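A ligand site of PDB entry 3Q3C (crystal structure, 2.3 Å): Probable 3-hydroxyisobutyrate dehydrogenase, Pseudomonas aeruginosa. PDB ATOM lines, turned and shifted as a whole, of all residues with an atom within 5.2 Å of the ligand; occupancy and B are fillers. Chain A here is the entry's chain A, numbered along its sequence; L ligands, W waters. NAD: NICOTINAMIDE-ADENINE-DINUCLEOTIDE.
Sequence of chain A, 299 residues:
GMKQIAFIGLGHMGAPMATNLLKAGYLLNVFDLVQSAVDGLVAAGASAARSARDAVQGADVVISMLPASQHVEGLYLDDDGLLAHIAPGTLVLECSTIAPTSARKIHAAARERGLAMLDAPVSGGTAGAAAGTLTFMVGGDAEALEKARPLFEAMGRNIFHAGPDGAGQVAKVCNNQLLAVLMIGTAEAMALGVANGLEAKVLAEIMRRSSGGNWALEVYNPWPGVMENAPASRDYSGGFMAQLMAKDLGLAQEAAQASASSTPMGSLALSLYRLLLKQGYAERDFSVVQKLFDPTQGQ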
ATOM      1  N   ILE A   8      24.597  -7.765 -22.216  1.00  0.00           N
ATOM      2  CA  ILE A   8      23.853  -6.663 -21.630  1.00  0.00           C
ATOM      3  C   ILE A   8      24.226  -5.328 -22.278  1.00  0.00           C
ATOM      4  O   ILE A   8      25.324  -4.827 -22.095  1.00  0.00           O
ATOM      5  CB  ILE A   8      24.103  -6.565 -20.102  1.00  0.00           C
ATOM      6  CG1 ILE A   8      23.268  -7.600 -19.355  1.00  0.00           C
ATOM      7  CG2 ILE A   8      23.755  -5.183 -19.595  1.00  0.00           C
ATOM      8  CD1 ILE A   8      23.716  -9.019 -19.569  1.00  0.00           C
ATOM      9  N   GLY A   9      23.290  -4.741 -23.010  1.00  0.00           N
ATOM     10  CA  GLY A   9      23.551  -3.516 -23.740  1.00  0.00           C
ATOM     11  C   GLY A   9      23.560  -3.833 -25.223  1.00  0.00           C
ATOM     12  O   GLY A   9      24.521  -4.393 -25.738  1.00  0.00           O
ATOM     13  N   LEU A  10      22.484  -3.480 -25.899  1.00  0.00           N
ATOM     14  CA  LEU A  10      22.310  -3.797 -27.306  1.00  0.00           C
ATOM     15  C   LEU A  10      22.063  -2.515 -28.104  1.00  0.00           C
ATOM     16  O   LEU A  10      21.073  -2.397 -28.803  1.00  0.00           O
ATOM     17  CB  LEU A  10      21.122  -4.743 -27.469  1.00  0.00           C
ATOM     18  CG  LEU A  10      21.124  -5.959 -26.538  1.00  0.00           C
ATOM     19  CD1 LEU A  10      19.830  -6.767 -26.692  1.00  0.00           C
ATOM     20  CD2 LEU A  10      22.326  -6.828 -26.770  1.00  0.00           C
ATOM     21  N   GLY A  11      22.969  -1.542 -27.977  1.00  0.00           N
ATOM     22  CA  GLY A  11      22.813  -0.269 -28.641  1.00  0.00           C
ATOM     23  C   GLY A  11      23.492  -0.311 -29.985  1.00  0.00           C
ATOM     24  O   GLY A  11      23.602  -1.365 -30.591  1.00  0.00           O
ATOM     25  N   HIS A  12      23.948   0.853 -30.443  1.00  0.00           N
ATOM     26  CA  HIS A  12      24.612   0.969 -31.751  1.00  0.00           C
ATOM     27  C   HIS A  12      25.750  -0.045 -31.944  1.00  0.00           C
ATOM     28  O   HIS A  12      25.990  -0.514 -33.049  1.00  0.00           O
ATOM     29  CB  HIS A  12      25.116   2.404 -31.968  1.00  0.00           C
ATOM     30  CG  HIS A  12      24.029   3.425 -32.019  1.00  0.00           C
ATOM     31  ND1 HIS A  12      22.778   3.162 -32.529  1.00  0.00           N
ATOM     32  CD2 HIS A  12      24.001   4.721 -31.621  1.00  0.00           C
ATOM     33  CE1 HIS A  12      22.028   4.238 -32.447  1.00  0.00           C
ATOM     34  NE2 HIS A  12      22.740   5.203 -31.900  1.00  0.00           N
ATOM     35  N   MET A  13      26.447  -0.359 -30.867  1.00  0.00           N
ATOM     36  CA  MET A  13      27.587  -1.248 -30.953  1.00  0.00           C
ATOM     37  C   MET A  13      27.204  -2.600 -30.381  1.00  0.00           C
ATOM     38  O   MET A  13      27.589  -3.633 -30.924  1.00  0.00           O
ATOM     39  CB  MET A  13      28.760  -0.663 -30.156  1.00  0.00           C
ATOM     40  CG  MET A  13      29.198   0.693 -30.655  1.00  0.00           C
ATOM     41  SD  MET A  13      30.144   0.540 -32.353  1.00  0.00           S
ATOM     42  CE  MET A  13      31.745  -0.379 -31.803  1.00  0.00           C
ATOM     43  N   GLY A  14      26.445  -2.579 -29.295  1.00  0.00           N
ATOM     44  CA  GLY A  14      25.987  -3.788 -28.639  1.00  0.00           C
ATOM     45  C   GLY A  14      25.219  -4.717 -29.548  1.00  0.00           C
ATOM     46  O   GLY A  14      25.522  -5.912 -29.647  1.00  0.00           O
ATOM     47  N   PHE A  31      19.886  -8.599 -22.712  1.00  0.00           N
ATOM     48  CA  PHE A  31      19.035  -7.644 -21.998  1.00  0.00           C
ATOM     49  C   PHE A  31      19.360  -6.184 -22.347  1.00  0.00           C
ATOM     50  O   PHE A  31      20.512  -5.836 -22.599  1.00  0.00           O
ATOM     51  CB  PHE A  31      19.071  -7.846 -20.472  1.00  0.00           C
ATOM     52  CG  PHE A  31      18.205  -6.857 -19.715  1.00  0.00           C
ATOM     53  CD1 PHE A  31      18.732  -5.649 -19.263  1.00  0.00           C
ATOM     54  CD2 PHE A  31      16.862  -7.124 -19.505  1.00  0.00           C
ATOM     55  CE1 PHE A  31      17.937  -4.729 -18.604  1.00  0.00           C
ATOM     56  CE2 PHE A  31      16.058  -6.206 -18.828  1.00  0.00           C
ATOM     57  CZ  PHE A  31      16.605  -5.020 -18.380  1.00  0.00           C
ATOM     58  N   ASP A  32      18.319  -5.349 -22.343  1.00  0.00           N
ATOM     59  CA  ASP A  32      18.494  -3.932 -22.673  1.00  0.00           C
ATOM     60  C   ASP A  32      17.270  -3.147 -22.238  1.00  0.00           C
ATOM     61  O   ASP A  32      16.144  -3.601 -22.394  1.00  0.00           O
ATOM     62  CB  ASP A  32      18.732  -3.783 -24.180  1.00  0.00           C
ATOM     63  CG  ASP A  32      19.257  -2.414 -24.554  1.00  0.00           C
ATOM     64  OD1 ASP A  32      20.483  -2.294 -24.753  1.00  0.00           O
ATOM     65  OD2 ASP A  32      18.452  -1.462 -24.675  1.00  0.00           O
ATOM     66  N   LEU A  33      17.492  -1.954 -21.694  1.00  0.00           N
ATOM     67  CA  LEU A  33      16.393  -1.127 -21.201  1.00  0.00           C
ATOM     68  C   LEU A  33      15.338  -0.869 -22.275  1.00  0.00           C
ATOM     69  O   LEU A  33      14.216  -0.464 -21.986  1.00  0.00           O
ATOM     70  CB  LEU A  33      16.942   0.211 -20.686  1.00  0.00           C
ATOM     71  CG  LEU A  33      17.500   0.357 -19.267  1.00  0.00           C
ATOM     72  CD1 LEU A  33      17.904  -0.962 -18.620  1.00  0.00           C
ATOM     73  CD2 LEU A  33      18.661   1.337 -19.293  1.00  0.00           C
ATOM     74  N   VAL A  34      15.717  -1.110 -23.527  1.00  0.00           N
ATOM     75  CA  VAL A  34      14.873  -0.775 -24.665  1.00  0.00           C
ATOM     76  C   VAL A  34      14.407  -2.035 -25.375  1.00  0.00           C
ATOM     77  O   VAL A  34      15.208  -2.764 -25.960  1.00  0.00           O
ATOM     78  CB  VAL A  34      15.632   0.116 -25.673  1.00  0.00           C
ATOM     79  CG1 VAL A  34      14.755   0.432 -26.864  1.00  0.00           C
ATOM     80  CG2 VAL A  34      16.076   1.395 -25.005  1.00  0.00           C
ATOM     81  N   ALA A  37      15.322  -3.163 -28.913  1.00  0.00           N
ATOM     82  CA  ALA A  37      16.678  -3.692 -29.055  1.00  0.00           C
ATOM     83  C   ALA A  37      16.756  -5.162 -28.638  1.00  0.00           C
ATOM     84  O   ALA A  37      17.440  -5.954 -29.280  1.00  0.00           O
ATOM     85  CB  ALA A  37      17.686  -2.839 -28.272  1.00  0.00           C
ATOM     86  N   MET A  65      28.106  -3.824 -22.980  1.00  0.00           N
ATOM     87  CA  MET A  65      28.441  -2.728 -23.881  1.00  0.00           C
ATOM     88  C   MET A  65      27.508  -1.538 -23.617  1.00  0.00           C
ATOM     89  O   MET A  65      26.500  -1.370 -24.307  1.00  0.00           O
ATOM     90  CB  MET A  65      28.328  -3.192 -25.344  1.00  0.00           C
ATOM     91  CG  MET A  65      28.863  -2.182 -26.359  1.00  0.00           C
ATOM     92  SD  MET A  65      30.722  -1.724 -26.001  1.00  0.00           S
ATOM     93  CE  MET A  65      31.247  -1.017 -27.739  1.00  0.00           C
ATOM     94  N   LEU A  66      27.823  -0.746 -22.605  1.00  0.00           N
ATOM     95  CA  LEU A  66      26.967   0.370 -22.177  1.00  0.00           C
ATOM     96  C   LEU A  66      27.636   1.719 -22.435  1.00  0.00           C
ATOM     97  O   LEU A  66      28.844   1.792 -22.706  1.00  0.00           O
ATOM     98  CB  LEU A  66      26.595   0.224 -20.691  1.00  0.00           C
ATOM     99  CG  LEU A  66      26.173  -1.154 -20.188  1.00  0.00           C
ATOM    100  CD1 LEU A  66      25.883  -1.156 -18.687  1.00  0.00           C
ATOM    101  CD2 LEU A  66      24.971  -1.649 -20.964  1.00  0.00           C
ATOM    102  N   PRO A  67      26.864   2.803 -22.329  1.00  0.00           N
ATOM    103  CA  PRO A  67      27.361   4.100 -22.806  1.00  0.00           C
ATOM    104  C   PRO A  67      28.479   4.733 -21.974  1.00  0.00           C
ATOM    105  O   PRO A  67      29.408   5.290 -22.581  1.00  0.00           O
ATOM    106  CB  PRO A  67      26.112   4.980 -22.799  1.00  0.00           C
ATOM    107  CG  PRO A  67      25.244   4.390 -21.726  1.00  0.00           C
ATOM    108  CD  PRO A  67      25.482   2.902 -21.807  1.00  0.00           C
ATOM    109  N   ALA A  68      28.422   4.684 -20.644  1.00  0.00           N
ATOM    110  CA  ALA A  68      29.396   5.435 -19.848  1.00  0.00           C
ATOM    111  C   ALA A  68      29.750   4.850 -18.472  1.00  0.00           C
ATOM    112  O   ALA A  68      29.254   3.782 -18.088  1.00  0.00           O
ATOM    113  CB  ALA A  68      28.959   6.883 -19.692  1.00  0.00           C
ATOM    114  N   HIS A  71      26.717   4.311 -15.789  1.00  0.00           N
ATOM    115  CA  HIS A  71      25.847   3.161 -16.023  1.00  0.00           C
ATOM    116  C   HIS A  71      26.555   1.872 -15.670  1.00  0.00           C
ATOM    117  O   HIS A  71      25.951   0.954 -15.106  1.00  0.00           O
ATOM    118  CB  HIS A  71      25.413   3.125 -17.477  1.00  0.00           C
ATOM    119  CG  HIS A  71      25.272   4.481 -18.099  1.00  0.00           C
ATOM    120  ND1 HIS A  71      26.345   5.215 -18.553  1.00  0.00           N
ATOM    121  CD2 HIS A  71      24.170   5.240 -18.340  1.00  0.00           C
ATOM    122  CE1 HIS A  71      25.921   6.357 -19.053  1.00  0.00           C
ATOM    123  NE2 HIS A  71      24.602   6.400 -18.935  1.00  0.00           N
ATOM    124  N   LEU A  75      25.584  -0.734 -12.754  1.00  0.00           N
ATOM    125  CA  LEU A  75      25.081  -2.076 -13.020  1.00  0.00           C
ATOM    126  C   LEU A  75      25.904  -3.173 -12.357  1.00  0.00           C
ATOM    127  O   LEU A  75      25.410  -4.270 -12.101  1.00  0.00           O
ATOM    128  CB  LEU A  75      24.974  -2.312 -14.517  1.00  0.00           C
ATOM    129  CG  LEU A  75      24.865  -3.785 -14.895  1.00  0.00           C
ATOM    130  CD1 LEU A  75      23.678  -4.020 -15.832  1.00  0.00           C
ATOM    131  CD2 LEU A  75      26.167  -4.260 -15.509  1.00  0.00           C
ATOM    132  N   CYS A  95      33.341  -4.274 -22.143  1.00  0.00           N
ATOM    133  CA  CYS A  95      33.722  -3.636 -23.422  1.00  0.00           C
ATOM    134  C   CYS A  95      33.269  -2.184 -23.579  1.00  0.00           C
ATOM    135  O   CYS A  95      33.534  -1.580 -24.605  1.00  0.00           O
ATOM    136  CB  CYS A  95      33.193  -4.455 -24.601  1.00  0.00           C
ATOM    137  SG  CYS A  95      33.815  -6.152 -24.685  1.00  0.00           S
ATOM    138  N   SER A  96      32.564  -1.631 -22.597  1.00  0.00           N
ATOM    139  CA  SER A  96      32.249  -0.205 -22.654  1.00  0.00           C
ATOM    140  C   SER A  96      33.546   0.592 -22.556  1.00  0.00           C
ATOM    141  O   SER A  96      34.567   0.059 -22.123  1.00  0.00           O
ATOM    142  CB  SER A  96      31.313   0.173 -21.507  1.00  0.00           C
ATOM    143  OG  SER A  96      30.251  -0.754 -21.413  1.00  0.00           O
ATOM    144  N   THR A  97      33.489   1.839 -22.992  1.00  0.00           N
ATOM    145  CA  THR A  97      34.586   2.772 -22.831  1.00  0.00           C
ATOM    146  C   THR A  97      34.273   3.601 -21.602  1.00  0.00           C
ATOM    147  O   THR A  97      33.333   4.401 -21.608  1.00  0.00           O
ATOM    148  CB  THR A  97      34.747   3.730 -24.042  1.00  0.00           C
ATOM    149  OG1 THR A  97      35.112   2.998 -25.210  1.00  0.00           O
ATOM    150  CG2 THR A  97      35.839   4.765 -23.768  1.00  0.00           C
ATOM    151  N   VAL A 122      36.309  -1.091 -27.188  1.00  0.00           N
ATOM    152  CA  VAL A 122      36.350  -1.266 -28.624  1.00  0.00           C
ATOM    153  C   VAL A 122      36.656   0.031 -29.378  1.00  0.00           C
ATOM    154  O   VAL A 122      36.187   1.121 -29.016  1.00  0.00           O
ATOM    155  CB  VAL A 122      35.015  -1.838 -29.128  1.00  0.00           C
ATOM    156  CG1 VAL A 122      34.705  -1.318 -30.501  1.00  0.00           C
ATOM    157  CG2 VAL A 122      35.062  -3.370 -29.108  1.00  0.00           C
ATOM    158  N   SER A 123      37.448  -0.100 -30.428  1.00  0.00           N
ATOM    159  CA  SER A 123      37.697   0.978 -31.365  1.00  0.00           C
ATOM    160  C   SER A 123      37.200   0.458 -32.702  1.00  0.00           C
ATOM    161  O   SER A 123      37.214  -0.741 -32.947  1.00  0.00           O
ATOM    162  CB  SER A 123      39.196   1.330 -31.361  1.00  0.00           C
ATOM    163  OG  SER A 123      39.552   2.223 -32.392  1.00  0.00           O
ATOM    164  N   GLY A 124      36.742   1.348 -33.558  1.00  0.00           N
ATOM    165  CA  GLY A 124      36.045   0.976 -34.784  1.00  0.00           C
ATOM    166  C   GLY A 124      34.705   1.671 -34.669  1.00  0.00           C
ATOM    167  O   GLY A 124      34.480   2.442 -33.730  1.00  0.00           O
ATOM    168  N   GLY A 125      33.796   1.436 -35.600  1.00  0.00           N
ATOM    169  CA  GLY A 125      32.480   2.019 -35.431  1.00  0.00           C
ATOM    170  C   GLY A 125      31.361   1.034 -35.633  1.00  0.00           C
ATOM    171  O   GLY A 125      31.556  -0.177 -35.652  1.00  0.00           O
ATOM    172  N   THR A 126      30.160   1.581 -35.782  1.00  0.00           N
ATOM    173  CA  THR A 126      28.962   0.828 -36.117  1.00  0.00           C
ATOM    174  C   THR A 126      29.172  -0.057 -37.338  1.00  0.00           C
ATOM    175  O   THR A 126      28.733  -1.209 -37.377  1.00  0.00           O
ATOM    176  CB  THR A 126      27.800   1.826 -36.367  1.00  0.00           C
ATOM    177  OG1 THR A 126      27.003   1.943 -35.173  1.00  0.00           O
ATOM    178  CG2 THR A 126      26.949   1.433 -37.583  1.00  0.00           C
ATOM    179  N   LYS A 172      42.699   3.017 -25.050  1.00  0.00           N
ATOM    180  CA  LYS A 172      41.547   3.511 -25.803  1.00  0.00           C
ATOM    181  C   LYS A 172      41.424   5.040 -25.715  1.00  0.00           C
ATOM    182  O   LYS A 172      41.315   5.749 -26.724  1.00  0.00           O
ATOM    183  CB  LYS A 172      40.275   2.857 -25.260  1.00  0.00           C
ATOM    184  CG  LYS A 172      38.990   3.361 -25.898  1.00  0.00           C
ATOM    185  CD  LYS A 172      38.967   3.174 -27.413  1.00  0.00           C
ATOM    186  CE  LYS A 172      37.750   3.898 -28.054  1.00  0.00           C
ATOM    187  NZ  LYS A 172      36.432   3.371 -27.584  1.00  0.00           N
ATOM    188  N   GLY A 239      27.936   7.600 -38.735  1.00  0.00           N
ATOM    189  CA  GLY A 239      29.283   7.556 -38.195  1.00  0.00           C
ATOM    190  C   GLY A 239      29.374   7.625 -36.673  1.00  0.00           C
ATOM    191  O   GLY A 239      28.482   7.191 -35.964  1.00  0.00           O
ATOM    192  N   PHE A 240      30.470   8.177 -36.191  1.00  0.00           N
ATOM    193  CA  PHE A 240      30.748   8.290 -34.760  1.00  0.00           C
ATOM    194  C   PHE A 240      30.355   9.685 -34.251  1.00  0.00           C
ATOM    195  O   PHE A 240      30.968  10.695 -34.640  1.00  0.00           O
ATOM    196  CB  PHE A 240      32.239   8.045 -34.536  1.00  0.00           C
ATOM    197  CG  PHE A 240      32.682   8.094 -33.097  1.00  0.00           C
ATOM    198  CD1 PHE A 240      33.699   8.942 -32.706  1.00  0.00           C
ATOM    199  CD2 PHE A 240      32.093   7.271 -32.141  1.00  0.00           C
ATOM    200  CE1 PHE A 240      34.123   8.979 -31.369  1.00  0.00           C
ATOM    201  CE2 PHE A 240      32.511   7.311 -30.818  1.00  0.00           C
ATOM    202  CZ  PHE A 240      33.534   8.170 -30.433  1.00  0.00           C
ATOM    203  N   LEU A 244      29.805  11.710 -28.545  1.00  0.00           N
ATOM    204  CA  LEU A 244      30.572  10.593 -27.980  1.00  0.00           C
ATOM    205  C   LEU A 244      32.057  10.931 -27.951  1.00  0.00           C
ATOM    206  O   LEU A 244      32.779  10.596 -27.000  1.00  0.00           O
ATOM    207  CB  LEU A 244      30.360   9.311 -28.780  1.00  0.00           C
ATOM    208  CG  LEU A 244      28.979   8.629 -28.622  1.00  0.00           C
ATOM    209  CD1 LEU A 244      28.761   7.569 -29.711  1.00  0.00           C
ATOM    210  CD2 LEU A 244      28.848   8.033 -27.222  1.00  0.00           C
ATOM    211  N   LYS A 247      32.794  12.944 -24.971  1.00  0.00           N
ATOM    212  CA  LYS A 247      32.796  12.091 -23.787  1.00  0.00           C
ATOM    213  C   LYS A 247      34.171  11.455 -23.607  1.00  0.00           C
ATOM    214  O   LYS A 247      34.789  11.564 -22.535  1.00  0.00           O
ATOM    215  CB  LYS A 247      31.721  11.010 -23.924  1.00  0.00           C
ATOM    216  CG  LYS A 247      31.514  10.171 -22.674  1.00  0.00           C
ATOM    217  CD  LYS A 247      32.228   8.835 -22.765  1.00  0.00           C
ATOM    218  CE  LYS A 247      31.667   7.946 -23.879  1.00  0.00           C
ATOM    219  NZ  LYS A 247      32.453   6.675 -24.026  1.00  0.00           N
ATOM    220  N   ASP A 248      34.654  10.805 -24.647  1.00  0.00           N
ATOM    221  CA  ASP A 248      36.008  10.224 -24.661  1.00  0.00           C
ATOM    222  C   ASP A 248      37.094  11.230 -24.270  1.00  0.00           C
ATOM    223  O   ASP A 248      37.981  10.919 -23.468  1.00  0.00           O
ATOM    224  CB  ASP A 248      36.315   9.601 -26.024  1.00  0.00           C
ATOM    225  CG  ASP A 248      35.521   8.320 -26.293  1.00  0.00           C
ATOM    226  OD1 ASP A 248      34.579   8.009 -25.514  1.00  0.00           O
ATOM    227  OD2 ASP A 248      35.843   7.601 -27.277  1.00  0.00           O
HETATM  228  PA  NAD L   1      24.512   3.039 -27.098  1.00  0.00           P
HETATM  229  O1A NAD L   1      23.927   4.212 -26.400  1.00  0.00           O
HETATM  230  O2A NAD L   1      24.110   3.067 -28.528  1.00  0.00           O
HETATM  231  O5B NAD L   1      24.023   1.643 -26.461  1.00  0.00           O
HETATM  232  C5B NAD L   1      24.043   1.405 -25.073  1.00  0.00           C
HETATM  233  C4B NAD L   1      22.967   0.388 -24.749  1.00  0.00           C
HETATM  234  O4B NAD L   1      23.063   0.019 -23.397  1.00  0.00           O
HETATM  235  C3B NAD L   1      21.560   0.950 -24.956  1.00  0.00           C
HETATM  236  O3B NAD L   1      20.826   0.173 -25.884  1.00  0.00           O
HETATM  237  C2B NAD L   1      20.906   0.883 -23.580  1.00  0.00           C
HETATM  238  O2B NAD L   1      19.582   0.416 -23.635  1.00  0.00           O
HETATM  239  C1B NAD L   1      21.772  -0.118 -22.837  1.00  0.00           C
HETATM  240  N9A NAD L   1      21.742   0.091 -21.368  1.00  0.00           N
HETATM  241  C8A NAD L   1      21.938   1.276 -20.703  1.00  0.00           C
HETATM  242  N7A NAD L   1      21.841   1.045 -19.373  1.00  0.00           N
HETATM  243  C5A NAD L   1      21.573  -0.269 -19.189  1.00  0.00           C
HETATM  244  C6A NAD L   1      21.380  -1.022 -18.034  1.00  0.00           C
HETATM  245  N6A NAD L   1      21.845  -0.540 -16.875  1.00  0.00           N
HETATM  246  N1A NAD L   1      21.120  -2.366 -18.154  1.00  0.00           N
HETATM  247  C2A NAD L   1      21.072  -2.964 -19.400  1.00  0.00           C
HETATM  248  N3A NAD L   1      21.256  -2.213 -20.537  1.00  0.00           N
HETATM  249  C4A NAD L   1      21.510  -0.876 -20.431  1.00  0.00           C
HETATM  250  O3  NAD L   1      26.107   3.064 -26.886  1.00  0.00           O
HETATM  251  PN  NAD L   1      27.077   2.456 -28.013  1.00  0.00           P
HETATM  252  O1N NAD L   1      27.059   3.405 -29.158  1.00  0.00           O
HETATM  253  O2N NAD L   1      26.676   1.020 -28.195  1.00  0.00           O
HETATM  254  O5D NAD L   1      28.553   2.577 -27.364  1.00  0.00           O
HETATM  255  C5D NAD L   1      28.836   2.081 -26.068  1.00  0.00           C
HETATM  256  C4D NAD L   1      30.266   2.418 -25.650  1.00  0.00           C
HETATM  257  O4D NAD L   1      31.153   2.097 -26.701  1.00  0.00           O
HETATM  258  C3D NAD L   1      30.465   3.893 -25.316  1.00  0.00           C
HETATM  259  O3D NAD L   1      31.137   3.967 -24.064  1.00  0.00           O
HETATM  260  C2D NAD L   1      31.265   4.418 -26.522  1.00  0.00           C
HETATM  261  O2D NAD L   1      32.174   5.479 -26.258  1.00  0.00           O
HETATM  262  C1D NAD L   1      31.987   3.188 -27.057  1.00  0.00           C
HETATM  263  N1N NAD L   1      32.140   3.213 -28.523  1.00  0.00           N
HETATM  264  C2N NAD L   1      31.156   3.752 -29.308  1.00  0.00           C
HETATM  265  C3N NAD L   1      31.284   3.786 -30.695  1.00  0.00           C
HETATM  266  C7N NAD L   1      30.099   4.150 -31.561  1.00  0.00           C
HETATM  267  O7N NAD L   1      30.324   4.544 -32.895  1.00  0.00           O
HETATM  268  N7N NAD L   1      28.848   4.075 -31.086  1.00  0.00           N
HETATM  269  C4N NAD L   1      32.444   3.266 -31.285  1.00  0.00           C
HETATM  270  C5N NAD L   1      33.441   2.714 -30.483  1.00  0.00           C
HETATM  271  C6N NAD L   1      33.278   2.691 -29.090  1.00  0.00           C
HETATM  272  O   HOH W   1      26.044   5.815 -29.752  1.00  0.00           O
HETATM  273  O   HOH W   2      34.495   5.269 -28.612  1.00  0.00           O
HETATM  274  O   HOH W   3      30.351   4.694 -35.333  1.00  0.00           O
HETATM  275  O   HOH W   4      34.050   0.596 -26.070  1.00  0.00           O
HETATM  276  O   HOH W   5      35.958   4.484 -31.646  1.00  0.00           O
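O of Thr 97 is in hydrogen-bond range of O3D of the ligand, at 3.3 Å. N of Gly 11 sits close to O3B of the ligand (3.5 Å). O2N of the ligand is in hydrogen-bond range of N of Met 13 (3.0 Å). The side-chain carboxylate (OD2) of Asp 32 lies within hydrogen-bond range of an oxygen (O2B) of the ligand (2.4 Å). The backbone carbonyl oxygen of Pro 67 lies within hydrogen-bond range of an oxygen (O3D) of the ligand. O2D of the ligand lies within hydrogen-bond range of NZ of Lys 247, 2.5 Å away. The backbone NH (N) of Thr 97 lies within hydrogen-bond range of an oxygen (O3D) of the ligand, at 3.3 Å. The backbone NH of His 12 sits at hydrogen-bond distance from an oxygen (O2A) of the ligand (2.9 Å). An oxygen (O3D) of the ligand sits close to the backbone carbonyl oxygen (O) of Leu 66, at 3.4 Å.
The backbone carbonyl oxygen (O) of Ile 8 sits at hydrogen-bond distance from the backbone NH (N) of Met 65 (3.1 Å). N of Thr 126 lies within hydrogen-bond range of SD of Met 13 (3.6 Å). The side-chain amino group (NZ) of Lys 172 sits at hydrogen-bond distance from the backbone carbonyl oxygen (O) of Val 122 (2.7 Å). The side-chain amino group of Lys 247 sits at hydrogen-bond distance from the backbone carbonyl oxygen of Thr 97, at 3.4 Å. OG1 of Thr 97 sits at hydrogen-bond distance from NZ of Lys 172. The backbone carbonyl oxygen of Phe 31 lies within hydrogen-bond range of the backbone NH of Gly 9, at 3.0 Å. OG of Ser 96 lies within hydrogen-bond range of N of Leu 66. The backbone carbonyl oxygen (O) of His 12 sits at hydrogen-bond distance from the side-chain hydroxyl (OG1) of Thr 126 (3.4 Å).
Residues that only touch the ligand: Ile 8 (3.5 Å), Gly 9 (3.6 Å), Leu 10 (3.7 Å), Gly 14 (3.8 Å), Phe 31 (3.6 Å), Leu 33 (3.2 Å), Val 34 (3.9 Å), Met 65 (3.3 Å), Leu 75 (3.8 Å), Val 122 (3.3 Å), Gly 124 (3.3 Å), Lys 172 (3.6 Å), Phe 240 (3.3 Å), Leu 244 (3.8 Å) and Asp 248 (3.6 Å). Hydrophobic or aromatic side chains that line the ligand: Ile 8, His 12, Met 13, Phe 31, Leu 33, Val 34, Met 65, Leu 66, Pro 67, Leu 75, Phe 240 and Leu 244. The nearest printed residue that does not touch the ligand is Thr 126 (4.1 Å).
Water W3 lies within hydrogen-bond range of O7N of the ligand (2.4 Å), N of Thr 126 (3.2 Å) and O of Gly 239 (3.2 Å). Water W2 lies within hydrogen-bond range of the side-chain amino group of Lys 172 (2.9 Å), the side-chain carboxylate of Asp 248 (3.0 Å) and an oxygen (O2D) of the ligand (3.3 Å). Water W4 lies within hydrogen-bond range of O of Cys 95 (2.7 Å), OG1 of Thr 97 (2.8 Å), N of Val 122 (3.0 Å) and O4D of the ligand (3.3 Å).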
